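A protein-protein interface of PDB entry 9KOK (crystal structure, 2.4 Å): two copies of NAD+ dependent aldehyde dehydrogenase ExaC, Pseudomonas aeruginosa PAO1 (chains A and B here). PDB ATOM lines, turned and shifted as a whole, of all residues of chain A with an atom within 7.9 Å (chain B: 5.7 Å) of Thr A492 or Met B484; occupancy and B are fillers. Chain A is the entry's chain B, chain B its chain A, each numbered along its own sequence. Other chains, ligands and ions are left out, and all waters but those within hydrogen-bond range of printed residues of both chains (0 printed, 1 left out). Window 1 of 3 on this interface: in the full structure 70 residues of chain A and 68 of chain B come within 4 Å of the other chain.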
ATOM      1  N   GLY A 138      -7.152  -4.311   6.550  1.00  0.00           N
ATOM      2  CA  GLY A 138      -8.351  -4.997   6.099  1.00  0.00           C
ATOM      3  C   GLY A 138      -8.063  -5.673   4.768  1.00  0.00           C
ATOM      4  O   GLY A 138      -6.907  -5.892   4.395  1.00  0.00           O
ATOM      5  N   SER A 139      -9.117  -5.973   4.019  1.00  0.00           N
ATOM      6  CA  SER A 139      -8.933  -6.769   2.818  1.00  0.00           C
ATOM      7  C   SER A 139      -9.666  -6.174   1.631  1.00  0.00           C
ATOM      8  O   SER A 139     -10.616  -5.392   1.760  1.00  0.00           O
ATOM      9  CB  SER A 139      -9.397  -8.229   2.973  1.00  0.00           C
ATOM     10  OG  SER A 139     -10.171  -8.447   4.118  1.00  0.00           O
ATOM     11  N   TYR A 150     -14.629  -5.275  -0.160  1.00  0.00           N
ATOM     12  CA  TYR A 150     -13.695  -4.590   0.725  1.00  0.00           C
ATOM     13  C   TYR A 150     -14.123  -4.843   2.164  1.00  0.00           C
ATOM     14  O   TYR A 150     -15.324  -4.851   2.466  1.00  0.00           O
ATOM     15  CB  TYR A 150     -13.637  -3.073   0.460  1.00  0.00           C
ATOM     16  CG  TYR A 150     -13.342  -2.699  -0.964  1.00  0.00           C
ATOM     17  CD1 TYR A 150     -12.027  -2.564  -1.411  1.00  0.00           C
ATOM     18  CD2 TYR A 150     -14.377  -2.512  -1.888  1.00  0.00           C
ATOM     19  CE1 TYR A 150     -11.736  -2.242  -2.740  1.00  0.00           C
ATOM     20  CE2 TYR A 150     -14.103  -2.171  -3.239  1.00  0.00           C
ATOM     21  CZ  TYR A 150     -12.778  -2.036  -3.648  1.00  0.00           C
ATOM     22  OH  TYR A 150     -12.487  -1.723  -4.961  1.00  0.00           O
ATOM     23  N   HIS A 151     -13.145  -5.094   3.039  1.00  0.00           N
ATOM     24  CA  HIS A 151     -13.370  -5.210   4.479  1.00  0.00           C
ATOM     25  C   HIS A 151     -12.485  -4.189   5.179  1.00  0.00           C
ATOM     26  O   HIS A 151     -11.254  -4.249   5.053  1.00  0.00           O
ATOM     27  CB  HIS A 151     -13.065  -6.629   4.965  1.00  0.00           C
ATOM     28  CG  HIS A 151     -13.902  -7.668   4.295  1.00  0.00           C
ATOM     29  ND1 HIS A 151     -13.552  -8.241   3.093  1.00  0.00           N
ATOM     30  CD2 HIS A 151     -15.091  -8.215   4.639  1.00  0.00           C
ATOM     31  CE1 HIS A 151     -14.486  -9.103   2.728  1.00  0.00           C
ATOM     32  NE2 HIS A 151     -15.433  -9.101   3.649  1.00  0.00           N
ATOM     33  N   ILE A 152     -13.110  -3.240   5.886  1.00  0.00           N
ATOM     34  CA  ILE A 152     -12.410  -2.140   6.546  1.00  0.00           C
ATOM     35  C   ILE A 152     -12.643  -2.264   8.045  1.00  0.00           C
ATOM     36  O   ILE A 152     -13.785  -2.457   8.483  1.00  0.00           O
ATOM     37  CB  ILE A 152     -12.876  -0.773   6.011  1.00  0.00           C
ATOM     38  CG1 ILE A 152     -12.301  -0.562   4.610  1.00  0.00           C
ATOM     39  CG2 ILE A 152     -12.426   0.359   6.916  1.00  0.00           C
ATOM     40  CD1 ILE A 152     -13.175   0.219   3.719  1.00  0.00           C
ATOM     41  N   HIS A 153     -11.561  -2.239   8.819  1.00  0.00           N
ATOM     42  CA  HIS A 153     -11.680  -2.260  10.274  1.00  0.00           C
ATOM     43  C   HIS A 153     -12.218  -0.924  10.754  1.00  0.00           C
ATOM     44  O   HIS A 153     -11.732   0.135  10.338  1.00  0.00           O
ATOM     45  CB  HIS A 153     -10.327  -2.532  10.951  1.00  0.00           C
ATOM     46  CG  HIS A 153      -9.674  -3.818  10.536  1.00  0.00           C
ATOM     47  ND1 HIS A 153      -9.955  -5.030  11.135  1.00  0.00           N
ATOM     48  CD2 HIS A 153      -8.738  -4.078   9.584  1.00  0.00           C
ATOM     49  CE1 HIS A 153      -9.235  -5.983  10.566  1.00  0.00           C
ATOM     50  NE2 HIS A 153      -8.486  -5.431   9.625  1.00  0.00           N
ATOM     51  N   GLU A 154     -13.213  -0.971  11.630  1.00  0.00           N
ATOM     52  CA  GLU A 154     -13.787   0.231  12.203  1.00  0.00           C
ATOM     53  C   GLU A 154     -13.789   0.137  13.721  1.00  0.00           C
ATOM     54  O   GLU A 154     -13.929  -0.955  14.284  1.00  0.00           O
ATOM     55  CB  GLU A 154     -15.214   0.455  11.690  1.00  0.00           C
ATOM     56  CG  GLU A 154     -15.294   0.596  10.195  1.00  0.00           C
ATOM     57  CD  GLU A 154     -16.654   1.102   9.724  1.00  0.00           C
ATOM     58  OE1 GLU A 154     -17.638   0.997  10.488  1.00  0.00           O
ATOM     59  OE2 GLU A 154     -16.746   1.606   8.587  1.00  0.00           O
ATOM     60  N   PRO A 155     -13.623   1.259  14.410  1.00  0.00           N
ATOM     61  CA  PRO A 155     -13.723   1.227  15.876  1.00  0.00           C
ATOM     62  C   PRO A 155     -15.119   0.805  16.295  1.00  0.00           C
ATOM     63  O   PRO A 155     -16.096   1.057  15.597  1.00  0.00           O
ATOM     64  CB  PRO A 155     -13.401   2.664  16.307  1.00  0.00           C
ATOM     65  CG  PRO A 155     -13.106   3.452  15.038  1.00  0.00           C
ATOM     66  CD  PRO A 155     -13.260   2.577  13.851  1.00  0.00           C
ATOM     67  N   LEU A 156     -15.211   0.104  17.425  1.00  0.00           N
ATOM     68  CA  LEU A 156     -16.537  -0.139  17.983  1.00  0.00           C
ATOM     69  C   LEU A 156     -17.172   1.154  18.500  1.00  0.00           C
ATOM     70  O   LEU A 156     -18.395   1.294  18.469  1.00  0.00           O
ATOM     71  CB  LEU A 156     -16.453  -1.185  19.090  1.00  0.00           C
ATOM     72  CG  LEU A 156     -16.288  -2.625  18.600  1.00  0.00           C
ATOM     73  CD1 LEU A 156     -15.831  -3.504  19.749  1.00  0.00           C
ATOM     74  CD2 LEU A 156     -17.594  -3.108  18.051  1.00  0.00           C
ATOM     75  N   ASP A 487      -9.498  -7.485  16.844  1.00  0.00           N
ATOM     76  CA  ASP A 487     -10.816  -7.784  16.322  1.00  0.00           C
ATOM     77  C   ASP A 487     -11.889  -7.796  17.396  1.00  0.00           C
ATOM     78  O   ASP A 487     -13.062  -7.606  17.069  1.00  0.00           O
ATOM     79  CB  ASP A 487     -10.756  -9.115  15.587  1.00  0.00           C
ATOM     80  CG  ASP A 487      -9.830  -9.048  14.373  1.00  0.00           C
ATOM     81  OD1 ASP A 487      -9.735  -7.946  13.757  1.00  0.00           O
ATOM     82  OD2 ASP A 487      -9.178 -10.076  14.063  1.00  0.00           O
ATOM     83  N   GLN A 490     -12.946  -3.999  17.338  1.00  0.00           N
ATOM     84  CA  GLN A 490     -13.307  -3.393  16.065  1.00  0.00           C
ATOM     85  C   GLN A 490     -14.475  -4.146  15.439  1.00  0.00           C
ATOM     86  O   GLN A 490     -14.741  -5.308  15.762  1.00  0.00           O
ATOM     87  CB  GLN A 490     -12.115  -3.373  15.080  1.00  0.00           C
ATOM     88  CG  GLN A 490     -10.880  -2.718  15.639  1.00  0.00           C
ATOM     89  CD  GLN A 490      -9.676  -2.856  14.703  1.00  0.00           C
ATOM     90  OE1 GLN A 490      -9.016  -1.854  14.349  1.00  0.00           O
ATOM     91  NE2 GLN A 490      -9.392  -4.089  14.296  1.00  0.00           N
ATOM     92  N   GLN A 491     -15.134  -3.477  14.497  1.00  0.00           N
ATOM     93  CA  GLN A 491     -16.179  -4.051  13.654  1.00  0.00           C
ATOM     94  C   GLN A 491     -15.636  -4.191  12.240  1.00  0.00           C
ATOM     95  O   GLN A 491     -14.825  -3.384  11.796  1.00  0.00           O
ATOM     96  CB  GLN A 491     -17.442  -3.145  13.591  1.00  0.00           C
ATOM     97  CG  GLN A 491     -18.501  -3.335  14.698  1.00  0.00           C
ATOM     98  CD  GLN A 491     -19.326  -4.627  14.487  1.00  0.00           C
ATOM     99  OE1 GLN A 491     -18.957  -5.508  13.695  1.00  0.00           O
ATOM    100  NE2 GLN A 491     -20.433  -4.736  15.198  1.00  0.00           N
ATOM    101  N   THR A 492     -16.111  -5.192  11.521  1.00  0.00           N
ATOM    102  CA  THR A 492     -15.748  -5.378  10.129  1.00  0.00           C
ATOM    103  C   THR A 492     -16.818  -4.733   9.257  1.00  0.00           C
ATOM    104  O   THR A 492     -17.979  -5.148   9.298  1.00  0.00           O
ATOM    105  CB  THR A 492     -15.611  -6.862   9.790  1.00  0.00           C
ATOM    106  OG1 THR A 492     -14.560  -7.418  10.575  1.00  0.00           O
ATOM    107  CG2 THR A 492     -15.288  -7.038   8.310  1.00  0.00           C
ATOM    108  N   LYS A 493     -16.425  -3.739   8.470  1.00  0.00           N
ATOM    109  CA  LYS A 493     -17.306  -3.105   7.499  1.00  0.00           C
ATOM    110  C   LYS A 493     -17.014  -3.722   6.141  1.00  0.00           C
ATOM    111  O   LYS A 493     -15.930  -3.520   5.588  1.00  0.00           O
ATOM    112  CB  LYS A 493     -17.076  -1.591   7.477  1.00  0.00           C
ATOM    113  CG  LYS A 493     -17.672  -0.838   6.273  1.00  0.00           C
ATOM    114  CD  LYS A 493     -19.214  -0.850   6.272  1.00  0.00           C
ATOM    115  CE  LYS A 493     -19.806  -0.307   7.596  1.00  0.00           C
ATOM    116  NZ  LYS A 493     -19.574   1.170   7.749  1.00  0.00           N
ATOM    117  N   ASN A 494     -17.985  -4.438   5.584  1.00  0.00           N
ATOM    118  CA  ASN A 494     -17.858  -5.017   4.246  1.00  0.00           C
ATOM    119  C   ASN A 494     -18.509  -4.072   3.219  1.00  0.00           C
ATOM    120  O   ASN A 494     -19.731  -3.996   3.121  1.00  0.00           O
ATOM    121  CB  ASN A 494     -18.499  -6.406   4.210  1.00  0.00           C
ATOM    122  CG  ASN A 494     -18.494  -7.035   2.802  1.00  0.00           C
ATOM    123  OD1 ASN A 494     -19.405  -7.775   2.457  1.00  0.00           O
ATOM    124  ND2 ASN A 494     -17.460  -6.760   2.007  1.00  0.00           N
ATOM    125  N   LEU A 495     -17.700  -3.348   2.446  1.00  0.00           N
ATOM    126  CA  LEU A 495     -18.208  -2.633   1.278  1.00  0.00           C
ATOM    127  C   LEU A 495     -18.197  -3.635   0.130  1.00  0.00           C
ATOM    128  O   LEU A 495     -17.134  -4.097  -0.280  1.00  0.00           O
ATOM    129  CB  LEU A 495     -17.372  -1.397   0.958  1.00  0.00           C
ATOM    130  CG  LEU A 495     -17.140  -0.461   2.159  1.00  0.00           C
ATOM    131  CD1 LEU A 495     -16.326   0.764   1.793  1.00  0.00           C
ATOM    132  CD2 LEU A 495     -18.482  -0.029   2.775  1.00  0.00           C
ATOM    133  N   TYR B 128     -15.863 -23.329  -0.953  1.00  0.00           N
ATOM    134  CA  TYR B 128     -15.127 -22.183  -0.439  1.00  0.00           C
ATOM    135  C   TYR B 128     -14.444 -22.531   0.870  1.00  0.00           C
ATOM    136  O   TYR B 128     -13.243 -22.283   1.042  1.00  0.00           O
ATOM    137  CB  TYR B 128     -16.060 -20.997  -0.252  1.00  0.00           C
ATOM    138  CG  TYR B 128     -15.414 -19.840   0.488  1.00  0.00           C
ATOM    139  CD1 TYR B 128     -14.538 -18.971  -0.169  1.00  0.00           C
ATOM    140  CD2 TYR B 128     -15.672 -19.613   1.835  1.00  0.00           C
ATOM    141  CE1 TYR B 128     -13.941 -17.914   0.490  1.00  0.00           C
ATOM    142  CE2 TYR B 128     -15.073 -18.551   2.509  1.00  0.00           C
ATOM    143  CZ  TYR B 128     -14.212 -17.694   1.807  1.00  0.00           C
ATOM    144  OH  TYR B 128     -13.615 -16.623   2.432  1.00  0.00           O
ATOM    145  N   ALA B 452     -23.527  -0.639   9.662  1.00  0.00           N
ATOM    146  CA  ALA B 452     -24.068  -1.930   9.245  1.00  0.00           C
ATOM    147  C   ALA B 452     -22.927  -2.832   8.808  1.00  0.00           C
ATOM    148  O   ALA B 452     -21.912  -2.360   8.306  1.00  0.00           O
ATOM    149  CB  ALA B 452     -25.088  -1.791   8.103  1.00  0.00           C
ATOM    150  N   GLY B 453     -23.111  -4.140   8.980  1.00  0.00           N
ATOM    151  CA  GLY B 453     -22.052  -5.071   8.626  1.00  0.00           C
ATOM    152  C   GLY B 453     -21.713  -5.057   7.146  1.00  0.00           C
ATOM    153  O   GLY B 453     -20.536  -5.086   6.772  1.00  0.00           O
ATOM    154  N   ARG B 454     -22.732  -4.976   6.282  1.00  0.00           N
ATOM    155  CA  ARG B 454     -22.526  -4.930   4.843  1.00  0.00           C
ATOM    156  C   ARG B 454     -23.178  -3.690   4.252  1.00  0.00           C
ATOM    157  O   ARG B 454     -24.353  -3.416   4.521  1.00  0.00           O
ATOM    158  CB  ARG B 454     -23.089  -6.161   4.133  1.00  0.00           C
ATOM    159  CG  ARG B 454     -22.862  -6.044   2.585  1.00  0.00           C
ATOM    160  CD  ARG B 454     -22.948  -7.386   1.876  1.00  0.00           C
ATOM    161  NE  ARG B 454     -21.962  -8.329   2.396  1.00  0.00           N
ATOM    162  CZ  ARG B 454     -22.047  -9.647   2.269  1.00  0.00           C
ATOM    163  NH1 ARG B 454     -23.054 -10.215   1.628  1.00  0.00           N
ATOM    164  NH2 ARG B 454     -21.091 -10.412   2.791  1.00  0.00           N
ATOM    165  N   ALA B 468     -17.593 -10.964   4.192  1.00  0.00           N
ATOM    166  CA  ALA B 468     -18.016 -11.212   5.573  1.00  0.00           C
ATOM    167  C   ALA B 468     -19.406 -10.643   5.843  1.00  0.00           C
ATOM    168  O   ALA B 468     -19.709  -9.508   5.468  1.00  0.00           O
ATOM    169  CB  ALA B 468     -17.038 -10.581   6.562  1.00  0.00           C
ATOM    170  N   TYR B 472     -23.882  -5.188  13.057  1.00  0.00           N
ATOM    171  CA  TYR B 472     -23.620  -4.137  14.033  1.00  0.00           C
ATOM    172  C   TYR B 472     -24.816  -4.062  14.976  1.00  0.00           C
ATOM    173  O   TYR B 472     -25.910  -4.532  14.645  1.00  0.00           O
ATOM    174  CB  TYR B 472     -23.460  -2.763  13.366  1.00  0.00           C
ATOM    175  CG  TYR B 472     -22.165  -2.453  12.661  1.00  0.00           C
ATOM    176  CD1 TYR B 472     -21.547  -3.377  11.803  1.00  0.00           C
ATOM    177  CD2 TYR B 472     -21.581  -1.198  12.806  1.00  0.00           C
ATOM    178  CE1 TYR B 472     -20.359  -3.053  11.137  1.00  0.00           C
ATOM    179  CE2 TYR B 472     -20.406  -0.865  12.166  1.00  0.00           C
ATOM    180  CZ  TYR B 472     -19.800  -1.784  11.328  1.00  0.00           C
ATOM    181  OH  TYR B 472     -18.632  -1.403  10.704  1.00  0.00           O
ATOM    182  N   ARG B 479     -19.303 -13.011  12.388  1.00  0.00           N
ATOM    183  CA  ARG B 479     -19.382 -12.903  10.939  1.00  0.00           C
ATOM    184  C   ARG B 479     -19.536 -14.287  10.327  1.00  0.00           C
ATOM    185  O   ARG B 479     -19.049 -15.283  10.881  1.00  0.00           O
ATOM    186  CB  ARG B 479     -18.146 -12.217  10.366  1.00  0.00           C
ATOM    187  CG  ARG B 479     -18.084 -10.739  10.670  1.00  0.00           C
ATOM    188  CD  ARG B 479     -19.249  -9.987  10.028  1.00  0.00           C
ATOM    189  NE  ARG B 479     -19.107  -8.543  10.203  1.00  0.00           N
ATOM    190  CZ  ARG B 479     -19.611  -7.884  11.239  1.00  0.00           C
ATOM    191  NH1 ARG B 479     -20.273  -8.513  12.195  1.00  0.00           N
ATOM    192  NH2 ARG B 479     -19.459  -6.564  11.312  1.00  0.00           N
ATOM    193  N   HIS B 482     -17.336 -16.084   5.169  1.00  0.00           N
ATOM    194  CA  HIS B 482     -15.976 -15.586   4.990  1.00  0.00           C
ATOM    195  C   HIS B 482     -15.028 -16.398   5.878  1.00  0.00           C
ATOM    196  O   HIS B 482     -15.397 -16.793   6.983  1.00  0.00           O
ATOM    197  CB  HIS B 482     -15.905 -14.091   5.348  1.00  0.00           C
ATOM    198  CG  HIS B 482     -14.564 -13.465   5.112  1.00  0.00           C
ATOM    199  ND1 HIS B 482     -13.499 -13.650   5.971  1.00  0.00           N
ATOM    200  CD2 HIS B 482     -14.108 -12.669   4.108  1.00  0.00           C
ATOM    201  CE1 HIS B 482     -12.440 -13.009   5.500  1.00  0.00           C
ATOM    202  NE2 HIS B 482     -12.786 -12.397   4.380  1.00  0.00           N
ATOM    203  N   LYS B 483     -13.810 -16.635   5.393  1.00  0.00           N
ATOM    204  CA  LYS B 483     -12.849 -17.468   6.119  1.00  0.00           C
ATOM    205  C   LYS B 483     -12.572 -16.967   7.538  1.00  0.00           C
ATOM    206  O   LYS B 483     -12.148 -17.748   8.395  1.00  0.00           O
ATOM    207  CB  LYS B 483     -11.539 -17.540   5.337  1.00  0.00           C
ATOM    208  CG  LYS B 483     -10.754 -16.219   5.342  1.00  0.00           C
ATOM    209  CD  LYS B 483      -9.484 -16.353   4.486  1.00  0.00           C
ATOM    210  CE  LYS B 483      -8.668 -15.053   4.494  1.00  0.00           C
ATOM    211  NZ  LYS B 483      -7.446 -15.203   3.680  1.00  0.00           N
ATOM    212  N   MET B 484     -12.746 -15.674   7.806  1.00  0.00           N
ATOM    213  CA  MET B 484     -12.568 -15.198   9.175  1.00  0.00           C
ATOM    214  C   MET B 484     -13.458 -15.967  10.163  1.00  0.00           C
ATOM    215  O   MET B 484     -13.110 -16.041  11.349  1.00  0.00           O
ATOM    216  CB  MET B 484     -12.797 -13.682   9.230  1.00  0.00           C
ATOM    217  CG  MET B 484     -14.287 -13.231   9.203  1.00  0.00           C
ATOM    218  SD  MET B 484     -14.472 -11.419   9.159  1.00  0.00           S
ATOM    219  CE  MET B 484     -13.854 -10.870  10.722  1.00  0.00           C
ATOM    220  N   MET B 485     -14.562 -16.585   9.689  1.00  0.00           N
ATOM    221  CA  MET B 485     -15.438 -17.387  10.552  1.00  0.00           C
ATOM    222  C   MET B 485     -14.743 -18.563  11.188  1.00  0.00           C
ATOM    223  O   MET B 485     -15.219 -19.055  12.216  1.00  0.00           O
ATOM    224  CB  MET B 485     -16.574 -18.075   9.805  1.00  0.00           C
ATOM    225  CG  MET B 485     -17.520 -17.355   9.001  1.00  0.00           C
ATOM    226  SD  MET B 485     -18.561 -18.740   8.519  1.00  0.00           S
ATOM    227  CE  MET B 485     -19.541 -18.832  10.043  1.00  0.00           C
ATOM    228  N   LEU B 486     -13.720 -19.111  10.526  1.00  0.00           N
ATOM    229  CA  LEU B 486     -13.066 -20.303  11.049  1.00  0.00           C
ATOM    230  C   LEU B 486     -12.656 -20.106  12.503  1.00  0.00           C
ATOM    231  O   LEU B 486     -12.757 -21.032  13.311  1.00  0.00           O
ATOM    232  CB  LEU B 486     -11.868 -20.652  10.160  1.00  0.00           C
ATOM    233  CG  LEU B 486     -12.329 -21.145   8.780  1.00  0.00           C
ATOM    234  CD1 LEU B 486     -11.174 -21.497   7.781  1.00  0.00           C
ATOM    235  CD2 LEU B 486     -13.267 -22.346   8.954  1.00  0.00           C
ATOM    236  N   ASP B 487     -12.342 -18.876  12.883  1.00  0.00           N
ATOM    237  CA  ASP B 487     -11.961 -18.617  14.258  1.00  0.00           C
ATOM    238  C   ASP B 487     -13.122 -18.730  15.228  1.00  0.00           C
ATOM    239  O   ASP B 487     -12.889 -18.968  16.418  1.00  0.00           O
ATOM    240  CB  ASP B 487     -11.305 -17.247  14.334  1.00  0.00           C
ATOM    241  CG  ASP B 487     -10.023 -17.204  13.520  1.00  0.00           C
ATOM    242  OD1 ASP B 487      -9.230 -18.176  13.629  1.00  0.00           O
ATOM    243  OD2 ASP B 487      -9.823 -16.231  12.764  1.00  0.00           O
ATOM    244  N   HIS B 488     -14.370 -18.535  14.771  1.00  0.00           N
ATOM    245  CA  HIS B 488     -15.509 -18.828  15.635  1.00  0.00           C
ATOM    246  C   HIS B 488     -15.638 -20.320  15.894  1.00  0.00           C
ATOM    247  O   HIS B 488     -16.336 -20.712  16.839  1.00  0.00           O
ATOM    248  CB  HIS B 488     -16.834 -18.350  15.012  1.00  0.00           C
ATOM    249  CG  HIS B 488     -16.941 -16.867  14.817  1.00  0.00           C
ATOM    250  ND1 HIS B 488     -16.690 -15.953  15.821  1.00  0.00           N
ATOM    251  CD2 HIS B 488     -17.282 -16.142  13.721  1.00  0.00           C
ATOM    252  CE1 HIS B 488     -16.870 -14.730  15.350  1.00  0.00           C
ATOM    253  NE2 HIS B 488     -17.227 -14.818  14.077  1.00  0.00           N
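Of the 14 printed residues of chain B, 8 touch a printed residue of chain A. Printed residues of chain B that touch a printed residue of chain A: Ala B452, Gly B453, Arg B454, Ala B468, Tyr B472, Arg B479, His B482 and Met B484. Hydrophobic or aromatic side chains of chain B within 4 Å of the printed part of chain A: Ala B468, Tyr B472, His B482 and Met B484. Along chain B the printed residues that touch a printed residue of chain A span positions 452 to 484. Hydrophobic or aromatic side chains of chain A that line the printed part of chain B: His A151. Among the printed residues, 15 pairs touch across the chains. Among the printed residues, no Asp or Glu carboxylate lies within 4 Å of a Lys or Arg side-chain nitrogen of the other chain.
1 position is printed for both chains.
Among the printed residues, pairs that only touch across the chains: His A151 with His B482 (3.8 Å), Gln A491 with Tyr B472 (3.4 Å), Thr A492 with Gly B453 (3.6 Å), Thr A492 with Tyr B472 (3.7 Å), Thr A492 with Met B484 (3.5 Å), Lys A493 with Ala B452 (3.0 Å), Lys A493 with Gly B453 (3.8 Å) and Lys A493 with Tyr B472 (3.5 Å).
A ring nitrogen (ND1) of His B482 sits at hydrogen-bond distance from the backbone NH (N) of Met B484 (2.8 Å). The backbone carbonyl oxygen (O) of Ser A139 lies within hydrogen-bond range of the backbone NH (N) of His A151 (2.8 Å). The backbone NH of Gln A491 lies within hydrogen-bond range of the backbone carbonyl oxygen of Glu A154 (2.8 Å). The guanidinium group of Arg B454 is in hydrogen-bond range of the backbone carbonyl oxygen of Ala B468, at 3.1 Å. N of Arg B479 lies within hydrogen-bond range of NE2 of His B488. The backbone carbonyl oxygen (O) of Lys A493 is in hydrogen-bond range of the backbone NH (N) of Ile A152 (2.8 Å).
Printed residues of chain B within 4 Å of Thr A492: Gly B453 (3.6 Å), Tyr B472 (3.7 Å), Arg B479 (2.9 Å) and Met B484 (3.5 Å). Of the printed residues of chain A, Tyr B472 touches Glu A154, Gln A491, Thr A492 and Lys A493. Of the printed residues of chain B, Lys A493 touches Ala B452, Gly B453 and Tyr B472. Printed residues of chain A within 4 Å of Arg B454: Asn A494 (2.6 Å). Ile A152 touches none of the printed residues of chain B. Asp A487 touches none of the printed residues of chain B. The nearest printed residue of chain A that does not touch Arg B479 is Lys A493 (5.0 Å).
O of Ala B468 sits close to OD1 of Asn A494 (3.5 Å). N of Ala B468 lies within hydrogen-bond range of NE2 of His A151 (2.9 Å). The side-chain hydroxyl (OH) of Tyr B472 is in hydrogen-bond range of the side-chain carboxylate (OE1) of Glu A154, at 2.6 Å. NH2 of Arg B479 is in hydrogen-bond range of O of Thr A492, at 2.9 Å. NE of Arg B454 sits at hydrogen-bond distance from OD1 of Asn A494 (2.6 Å). NH2 of Arg B479 sits at hydrogen-bond distance from OE1 of Gln A491 (2.7 Å). O of Gly B453 lies within hydrogen-bond range of N of Asn A494 (2.9 Å).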
